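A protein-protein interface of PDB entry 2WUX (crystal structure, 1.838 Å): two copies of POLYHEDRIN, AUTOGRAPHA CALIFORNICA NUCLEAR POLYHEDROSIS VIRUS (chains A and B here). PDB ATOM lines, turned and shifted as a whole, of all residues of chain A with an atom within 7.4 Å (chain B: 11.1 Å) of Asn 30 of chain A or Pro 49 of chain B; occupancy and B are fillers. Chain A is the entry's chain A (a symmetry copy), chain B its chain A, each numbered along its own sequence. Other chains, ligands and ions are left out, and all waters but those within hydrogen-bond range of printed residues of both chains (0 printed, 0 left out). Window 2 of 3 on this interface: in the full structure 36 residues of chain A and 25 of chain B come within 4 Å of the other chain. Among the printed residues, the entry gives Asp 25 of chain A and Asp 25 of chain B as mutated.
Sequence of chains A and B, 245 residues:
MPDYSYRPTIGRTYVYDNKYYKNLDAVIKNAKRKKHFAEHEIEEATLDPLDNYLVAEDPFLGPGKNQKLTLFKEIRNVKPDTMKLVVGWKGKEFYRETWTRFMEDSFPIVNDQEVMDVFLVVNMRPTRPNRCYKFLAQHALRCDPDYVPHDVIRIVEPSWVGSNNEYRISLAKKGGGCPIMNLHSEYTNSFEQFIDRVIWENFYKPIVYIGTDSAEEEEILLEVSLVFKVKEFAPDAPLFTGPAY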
ATOM      1  N   LYS A  22     -13.715 -23.770   9.996  1.00  0.00           N
ATOM      2  CA  LYS A  22     -13.819 -24.883  10.926  1.00  0.00           C
ATOM      3  C   LYS A  22     -15.158 -25.575  10.719  1.00  0.00           C
ATOM      4  O   LYS A  22     -16.121 -24.933  10.295  1.00  0.00           O
ATOM      5  CB  LYS A  22     -13.697 -24.394  12.373  1.00  0.00           C
ATOM      6  CG  LYS A  22     -13.725 -25.522  13.399  1.00  0.00           C
ATOM      7  CD  LYS A  22     -13.504 -25.024  14.819  1.00  0.00           C
ATOM      8  CE  LYS A  22     -13.480 -26.183  15.807  1.00  0.00           C
ATOM      9  NZ  LYS A  22     -12.401 -27.159  15.481  1.00  0.00           N
ATOM     10  N   ASP A  25     -20.265 -28.545  13.278  1.00  0.00           N
ATOM     11  CA  ASP A  25     -20.625 -29.350  14.443  1.00  0.00           C
ATOM     12  C   ASP A  25     -19.662 -29.113  15.606  1.00  0.00           C
ATOM     13  O   ASP A  25     -20.076 -29.090  16.764  1.00  0.00           O
ATOM     14  CB  ASP A  25     -20.678 -30.840  14.088  1.00  0.00           C
ATOM     15  CG  ASP A  25     -19.368 -31.350  13.516  1.00  0.00           C
ATOM     16  OD1 ASP A  25     -18.749 -30.629  12.702  1.00  0.00           O
ATOM     17  OD2 ASP A  25     -18.963 -32.480  13.870  1.00  0.00           O
ATOM     18  N   ALA A  26     -18.382 -28.932  15.291  1.00  0.00           N
ATOM     19  CA  ALA A  26     -17.366 -28.696  16.315  1.00  0.00           C
ATOM     20  C   ALA A  26     -17.450 -27.278  16.884  1.00  0.00           C
ATOM     21  O   ALA A  26     -17.035 -27.028  18.018  1.00  0.00           O
ATOM     22  CB  ALA A  26     -15.976 -28.962  15.758  1.00  0.00           C
ATOM     23  N   VAL A  27     -17.979 -26.352  16.089  1.00  0.00           N
ATOM     24  CA  VAL A  27     -18.175 -24.978  16.539  1.00  0.00           C
ATOM     25  C   VAL A  27     -19.398 -24.885  17.451  1.00  0.00           C
ATOM     26  O   VAL A  27     -19.380 -24.179  18.461  1.00  0.00           O
ATOM     27  CB  VAL A  27     -18.310 -24.004  15.344  1.00  0.00           C
ATOM     28  CG1 VAL A  27     -18.977 -22.698  15.773  1.00  0.00           C
ATOM     29  CG2 VAL A  27     -16.945 -23.742  14.717  1.00  0.00           C
ATOM     30  N   ILE A  28     -20.452 -25.615  17.090  1.00  0.00           N
ATOM     31  CA  ILE A  28     -21.661 -25.708  17.904  1.00  0.00           C
ATOM     32  C   ILE A  28     -21.347 -26.328  19.263  1.00  0.00           C
ATOM     33  O   ILE A  28     -21.649 -25.745  20.304  1.00  0.00           O
ATOM     34  CB  ILE A  28     -22.756 -26.539  17.197  1.00  0.00           C
ATOM     35  CG1 ILE A  28     -23.676 -25.631  16.382  1.00  0.00           C
ATOM     36  CG2 ILE A  28     -23.579 -27.318  18.212  1.00  0.00           C
ATOM     37  CD1 ILE A  28     -22.952 -24.721  15.421  1.00  0.00           C
ATOM     38  N   LYS A  29     -20.738 -27.509  19.249  1.00  0.00           N
ATOM     39  CA  LYS A  29     -20.291 -28.147  20.479  1.00  0.00           C
ATOM     40  C   LYS A  29     -19.046 -27.427  20.997  1.00  0.00           C
ATOM     41  O   LYS A  29     -17.918 -27.846  20.737  1.00  0.00           O
ATOM     42  CB  LYS A  29     -19.997 -29.631  20.243  1.00  0.00           C
ATOM     43  CG  LYS A  29     -19.675 -30.411  21.510  1.00  0.00           C
ATOM     44  CD  LYS A  29     -19.321 -31.861  21.199  1.00  0.00           C
ATOM     45  CE  LYS A  29     -18.938 -32.624  22.462  1.00  0.00           C
ATOM     46  NZ  LYS A  29     -18.481 -34.012  22.164  1.00  0.00           N
ATOM     47  N   ASN A  30     -19.264 -26.334  21.723  1.00  0.00           N
ATOM     48  CA  ASN A  30     -18.170 -25.516  22.236  1.00  0.00           C
ATOM     49  C   ASN A  30     -18.245 -25.361  23.756  1.00  0.00           C
ATOM     50  O   ASN A  30     -17.337 -24.810  24.382  1.00  0.00           O
ATOM     51  CB  ASN A  30     -18.178 -24.142  21.556  1.00  0.00           C
ATOM     52  CG  ASN A  30     -16.796 -23.525  21.462  1.00  0.00           C
ATOM     53  OD1 ASN A  30     -15.905 -23.842  22.251  1.00  0.00           O
ATOM     54  ND2 ASN A  30     -16.612 -22.635  20.493  1.00  0.00           N
ATOM     55  N   ALA A  31     -19.333 -25.856  24.341  1.00  0.00           N
ATOM     56  CA  ALA A  31     -19.528 -25.813  25.787  1.00  0.00           C
ATOM     57  C   ALA A  31     -20.806 -26.545  26.186  1.00  0.00           C
ATOM     58  O   ALA A  31     -20.857 -27.776  26.185  1.00  0.00           O
ATOM     59  CB  ALA A  31     -19.564 -24.374  26.278  1.00  0.00           C
ATOM     60  N   LEU A  61     -10.719 -11.862  14.348  1.00  0.00           N
ATOM     61  CA  LEU A  61     -10.533 -12.774  15.478  1.00  0.00           C
ATOM     62  C   LEU A  61      -9.653 -13.969  15.100  1.00  0.00           C
ATOM     63  O   LEU A  61      -9.145 -14.682  15.968  1.00  0.00           O
ATOM     64  CB  LEU A  61     -11.887 -13.251  16.027  1.00  0.00           C
ATOM     65  CG  LEU A  61     -12.892 -12.177  16.488  1.00  0.00           C
ATOM     66  CD1 LEU A  61     -14.159 -12.816  17.039  1.00  0.00           C
ATOM     67  CD2 LEU A  61     -12.278 -11.245  17.527  1.00  0.00           C
ATOM     68  N   TYR B   6     -19.366  -8.003  29.541  1.00  0.00           N
ATOM     69  CA  TYR B   6     -20.352  -7.894  28.468  1.00  0.00           C
ATOM     70  C   TYR B   6     -21.057  -9.230  28.222  1.00  0.00           C
ATOM     71  O   TYR B   6     -20.429 -10.287  28.281  1.00  0.00           O
ATOM     72  CB  TYR B   6     -19.694  -7.395  27.192  1.00  0.00           C
ATOM     73  N   ARG B   7     -22.356  -9.182  27.936  1.00  0.00           N
ATOM     74  CA  ARG B   7     -23.157 -10.401  27.808  1.00  0.00           C
ATOM     75  C   ARG B   7     -24.051 -10.531  26.560  1.00  0.00           C
ATOM     76  O   ARG B   7     -24.569 -11.617  26.296  1.00  0.00           O
ATOM     77  CB  ARG B   7     -23.984 -10.625  29.075  1.00  0.00           C
ATOM     78  N   PRO B   8     -24.258  -9.437  25.803  1.00  0.00           N
ATOM     79  CA  PRO B   8     -25.083  -9.558  24.594  1.00  0.00           C
ATOM     80  C   PRO B   8     -24.243  -9.743  23.334  1.00  0.00           C
ATOM     81  O   PRO B   8     -23.040  -9.484  23.353  1.00  0.00           O
ATOM     82  CB  PRO B   8     -25.799  -8.201  24.519  1.00  0.00           C
ATOM     83  CG  PRO B   8     -25.307  -7.396  25.714  1.00  0.00           C
ATOM     84  CD  PRO B   8     -24.027  -8.026  26.139  1.00  0.00           C
ATOM     85  N   THR B   9     -24.877 -10.172  22.248  1.00  0.00           N
ATOM     86  CA  THR B   9     -24.173 -10.353  20.982  1.00  0.00           C
ATOM     87  C   THR B   9     -24.418  -9.179  20.037  1.00  0.00           C
ATOM     88  O   THR B   9     -25.544  -8.697  19.905  1.00  0.00           O
ATOM     89  CB  THR B   9     -24.571 -11.673  20.283  1.00  0.00           C
ATOM     90  OG1 THR B   9     -25.981 -11.680  20.026  1.00  0.00           O
ATOM     91  CG2 THR B   9     -24.209 -12.868  21.154  1.00  0.00           C
ATOM     92  N   ARG B  12     -21.988  -8.084  13.196  1.00  0.00           N
ATOM     93  CA  ARG B  12     -20.898  -7.536  12.408  1.00  0.00           C
ATOM     94  C   ARG B  12     -20.911  -8.138  11.014  1.00  0.00           C
ATOM     95  O   ARG B  12     -21.317  -9.286  10.819  1.00  0.00           O
ATOM     96  CB  ARG B  12     -19.548  -7.739  13.103  1.00  0.00           C
ATOM     97  CG  ARG B  12     -18.917  -9.096  12.914  1.00  0.00           C
ATOM     98  CD  ARG B  12     -17.730  -9.260  13.863  1.00  0.00           C
ATOM     99  NE  ARG B  12     -18.164  -9.555  15.226  1.00  0.00           N
ATOM    100  CZ  ARG B  12     -18.222 -10.780  15.737  1.00  0.00           C
ATOM    101  NH1 ARG B  12     -18.636 -10.968  16.982  1.00  0.00           N
ATOM    102  NH2 ARG B  12     -17.862 -11.821  14.999  1.00  0.00           N
ATOM    103  N   LYS B  22     -22.037 -12.437   7.758  1.00  0.00           N
ATOM    104  CA  LYS B  22     -22.454 -11.936   9.059  1.00  0.00           C
ATOM    105  C   LYS B  22     -22.028 -12.929  10.129  1.00  0.00           C
ATOM    106  O   LYS B  22     -21.919 -14.124   9.849  1.00  0.00           O
ATOM    107  CB  LYS B  22     -23.972 -11.734   9.100  1.00  0.00           C
ATOM    108  CG  LYS B  22     -24.468 -11.141  10.415  1.00  0.00           C
ATOM    109  CD  LYS B  22     -25.963 -10.858  10.398  1.00  0.00           C
ATOM    110  CE  LYS B  22     -26.411 -10.212  11.704  1.00  0.00           C
ATOM    111  NZ  LYS B  22     -25.695  -8.929  11.954  1.00  0.00           N
ATOM    112  N   ASN B  23     -21.802 -12.449  11.351  1.00  0.00           N
ATOM    113  CA  ASN B  23     -21.393 -13.336  12.442  1.00  0.00           C
ATOM    114  C   ASN B  23     -22.508 -14.288  12.840  1.00  0.00           C
ATOM    115  O   ASN B  23     -23.678 -13.907  12.896  1.00  0.00           O
ATOM    116  CB  ASN B  23     -20.881 -12.564  13.660  1.00  0.00           C
ATOM    117  CG  ASN B  23     -21.901 -11.600  14.208  1.00  0.00           C
ATOM    118  OD1 ASN B  23     -22.642 -10.968  13.455  1.00  0.00           O
ATOM    119  ND2 ASN B  23     -21.936 -11.465  15.529  1.00  0.00           N
ATOM    120  N   LEU B  24     -22.119 -15.527  13.124  1.00  0.00           N
ATOM    121  CA  LEU B  24     -23.049 -16.631  13.330  1.00  0.00           C
ATOM    122  C   LEU B  24     -23.933 -16.430  14.560  1.00  0.00           C
ATOM    123  O   LEU B  24     -25.132 -16.699  14.513  1.00  0.00           O
ATOM    124  CB  LEU B  24     -22.276 -17.951  13.427  1.00  0.00           C
ATOM    125  CG  LEU B  24     -23.071 -19.257  13.483  1.00  0.00           C
ATOM    126  CD1 LEU B  24     -23.932 -19.434  12.231  1.00  0.00           C
ATOM    127  CD2 LEU B  24     -22.128 -20.435  13.670  1.00  0.00           C
ATOM    128  N   ASP B  25     -23.347 -15.958  15.655  1.00  0.00           N
ATOM    129  CA  ASP B  25     -24.108 -15.759  16.887  1.00  0.00           C
ATOM    130  C   ASP B  25     -25.243 -14.755  16.688  1.00  0.00           C
ATOM    131  O   ASP B  25     -26.327 -14.918  17.245  1.00  0.00           O
ATOM    132  CB  ASP B  25     -23.194 -15.314  18.034  1.00  0.00           C
ATOM    133  CG  ASP B  25     -22.431 -14.043  17.712  1.00  0.00           C
ATOM    134  OD1 ASP B  25     -21.952 -13.907  16.564  1.00  0.00           O
ATOM    135  OD2 ASP B  25     -22.298 -13.184  18.612  1.00  0.00           O
ATOM    136  N   ALA B  26     -24.989 -13.721  15.888  1.00  0.00           N
ATOM    137  CA  ALA B  26     -25.993 -12.695  15.619  1.00  0.00           C
ATOM    138  C   ALA B  26     -27.079 -13.196  14.665  1.00  0.00           C
ATOM    139  O   ALA B  26     -28.207 -12.698  14.676  1.00  0.00           O
ATOM    140  CB  ALA B  26     -25.338 -11.440  15.065  1.00  0.00           C
ATOM    141  N   ILE B  28     -28.011 -16.505  14.605  1.00  0.00           N
ATOM    142  CA  ILE B  28     -28.755 -17.411  15.475  1.00  0.00           C
ATOM    143  C   ILE B  28     -29.749 -16.636  16.335  1.00  0.00           C
ATOM    144  O   ILE B  28     -30.944 -16.931  16.336  1.00  0.00           O
ATOM    145  CB  ILE B  28     -27.808 -18.226  16.385  1.00  0.00           C
ATOM    146  CG1 ILE B  28     -27.446 -19.557  15.728  1.00  0.00           C
ATOM    147  CG2 ILE B  28     -28.456 -18.487  17.738  1.00  0.00           C
ATOM    148  CD1 ILE B  28     -26.902 -19.426  14.327  1.00  0.00           C
ATOM    149  N   PRO B  49     -16.294 -19.905  20.824  1.00  0.00           N
ATOM    150  CA  PRO B  49     -17.643 -19.328  20.879  1.00  0.00           C
ATOM    151  C   PRO B  49     -18.203 -19.072  19.481  1.00  0.00           C
ATOM    152  O   PRO B  49     -17.435 -18.793  18.556  1.00  0.00           O
ATOM    153  CB  PRO B  49     -17.431 -17.996  21.616  1.00  0.00           C
ATOM    154  CG  PRO B  49     -15.956 -17.728  21.535  1.00  0.00           C
ATOM    155  CD  PRO B  49     -15.310 -19.075  21.539  1.00  0.00           C
ATOM    156  N   LEU B  50     -19.523 -19.162  19.338  1.00  0.00           N
ATOM    157  CA  LEU B  50     -20.175 -18.996  18.042  1.00  0.00           C
ATOM    158  C   LEU B  50     -19.847 -17.660  17.388  1.00  0.00           C
ATOM    159  O   LEU B  50     -19.699 -17.579  16.167  1.00  0.00           O
ATOM    160  CB  LEU B  50     -21.693 -19.142  18.177  1.00  0.00           C
ATOM    161  CG  LEU B  50     -22.297 -20.453  17.674  1.00  0.00           C
ATOM    162  CD1 LEU B  50     -21.482 -21.643  18.156  1.00  0.00           C
ATOM    163  CD2 LEU B  50     -23.745 -20.570  18.115  1.00  0.00           C
ATOM    164  N   ASP B  51     -19.744 -16.618  18.209  1.00  0.00           N
ATOM    165  CA  ASP B  51     -19.506 -15.263  17.716  1.00  0.00           C
ATOM    166  C   ASP B  51     -18.234 -15.140  16.889  1.00  0.00           C
ATOM    167  O   ASP B  51     -18.101 -14.224  16.085  1.00  0.00           O
ATOM    168  CB  ASP B  51     -19.513 -14.217  18.851  1.00  0.00           C
ATOM    169  CG  ASP B  51     -19.379 -14.829  20.248  1.00  0.00           C
ATOM    170  OD1 ASP B  51     -19.395 -14.049  21.226  1.00  0.00           O
ATOM    171  OD2 ASP B  51     -19.262 -16.065  20.387  1.00  0.00           O
ATOM    172  N   ASN B  52     -17.306 -16.068  17.089  1.00  0.00           N
ATOM    173  CA  ASN B  52     -16.038 -16.049  16.370  1.00  0.00           C
ATOM    174  C   ASN B  52     -16.154 -16.460  14.903  1.00  0.00           C
ATOM    175  O   ASN B  52     -15.160 -16.433  14.177  1.00  0.00           O
ATOM    176  CB  ASN B  52     -15.023 -16.964  17.057  1.00  0.00           C
ATOM    177  CG  ASN B  52     -14.598 -16.448  18.414  1.00  0.00           C
ATOM    178  OD1 ASN B  52     -15.158 -15.478  18.927  1.00  0.00           O
ATOM    179  ND2 ASN B  52     -13.603 -17.097  19.005  1.00  0.00           N
ATOM    180  N   TYR B  53     -17.355 -16.850  14.472  1.00  0.00           N
ATOM    181  CA  TYR B  53     -17.524 -17.426  13.138  1.00  0.00           C
ATOM    182  C   TYR B  53     -18.570 -16.718  12.281  1.00  0.00           C
ATOM    183  O   TYR B  53     -19.510 -16.126  12.801  1.00  0.00           O
ATOM    184  CB  TYR B  53     -17.834 -18.917  13.258  1.00  0.00           C
ATOM    185  CG  TYR B  53     -16.700 -19.653  13.921  1.00  0.00           C
ATOM    186  CD1 TYR B  53     -15.634 -20.143  13.174  1.00  0.00           C
ATOM    187  CD2 TYR B  53     -16.666 -19.818  15.300  1.00  0.00           C
ATOM    188  CE1 TYR B  53     -14.578 -20.798  13.779  1.00  0.00           C
ATOM    189  CE2 TYR B  53     -15.617 -20.473  15.908  1.00  0.00           C
ATOM    190  CZ  TYR B  53     -14.577 -20.957  15.144  1.00  0.00           C
ATOM    191  OH  TYR B  53     -13.535 -21.606  15.754  1.00  0.00           O
ATOM    192  N   LEU B  54     -18.390 -16.795  10.966  1.00  0.00           N
ATOM    193  CA  LEU B  54     -19.229 -16.079  10.006  1.00  0.00           C
ATOM    194  C   LEU B  54     -19.983 -17.028   9.091  1.00  0.00           C
ATOM    195  O   LEU B  54     -19.503 -18.120   8.769  1.00  0.00           O
ATOM    196  CB  LEU B  54     -18.369 -15.178   9.106  1.00  0.00           C
ATOM    197  CG  LEU B  54     -17.419 -14.168   9.739  1.00  0.00           C
ATOM    198  CD1 LEU B  54     -16.793 -13.315   8.648  1.00  0.00           C
ATOM    199  CD2 LEU B  54     -18.152 -13.303  10.750  1.00  0.00           C
ATOM    200  N   VAL B  55     -21.159 -16.587   8.656  1.00  0.00           N
ATOM    201  CA  VAL B  55     -21.903 -17.265   7.611  1.00  0.00           C
ATOM    202  C   VAL B  55     -22.147 -16.281   6.460  1.00  0.00           C
ATOM    203  O   VAL B  55     -22.276 -15.085   6.688  1.00  0.00           O
ATOM    204  CB  VAL B  55     -23.248 -17.805   8.146  1.00  0.00           C
ATOM    205  CG1 VAL B  55     -24.070 -16.683   8.775  1.00  0.00           C
ATOM    206  CG2 VAL B  55     -24.025 -18.458   7.040  1.00  0.00           C
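ND2 of Asn 30 of chain A sits close to N of Pro 49 of chain B, 2.8 Å away.
N of Leu 24 of chain B lies within hydrogen-bond range of O of Tyr 53 of chain B, at 2.7 Å.
Among the printed residues, pairs that only touch across the chains: Val 27 of chain A with Leu 50 of chain B, Leu 61 of chain A with Asn 52 of chain B, Lys 22 of chain A with Tyr 53 of chain B and Val 27 of chain A with Tyr 53 of chain B.
Printed residues of chain B within 4 Å of Lys 22 of chain A: Tyr 53.
Of chain B, only Pro 49 comes within 4 Å of Asn 30 of chain A.
No residue of chain B comes within 4 Å of Ala 31 of chain A.
Of the printed residues of chain B, Leu 61 of chain A touches Asn 52 (3.4 Å).
Leu 24 of chain B touches none of the printed residues of chain A.
Asp 25 of chain B touches none of the printed residues of chain A.
Pro 49 of chain B touches just one residue of chain A: Asn 30 (2.8 Å).
Of the printed residues of chain A, Tyr 53 of chain B touches Lys 22 and Val 27.
The nearest residue of chain A that does not touch Pro 49 of chain B is Val 27 of chain A (5.0 Å).
Hydrophobic or aromatic side chains of chain B within 4 Å of the printed part of chain A: Pro 49, Leu 50 and Tyr 53.
Of the 9 printed residues of chain A, 4 touch a printed residue of chain B.
Among the printed residues, 5 pairs touch across the chains.
Positions printed for both chains: 22, 25, 26 and 28.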
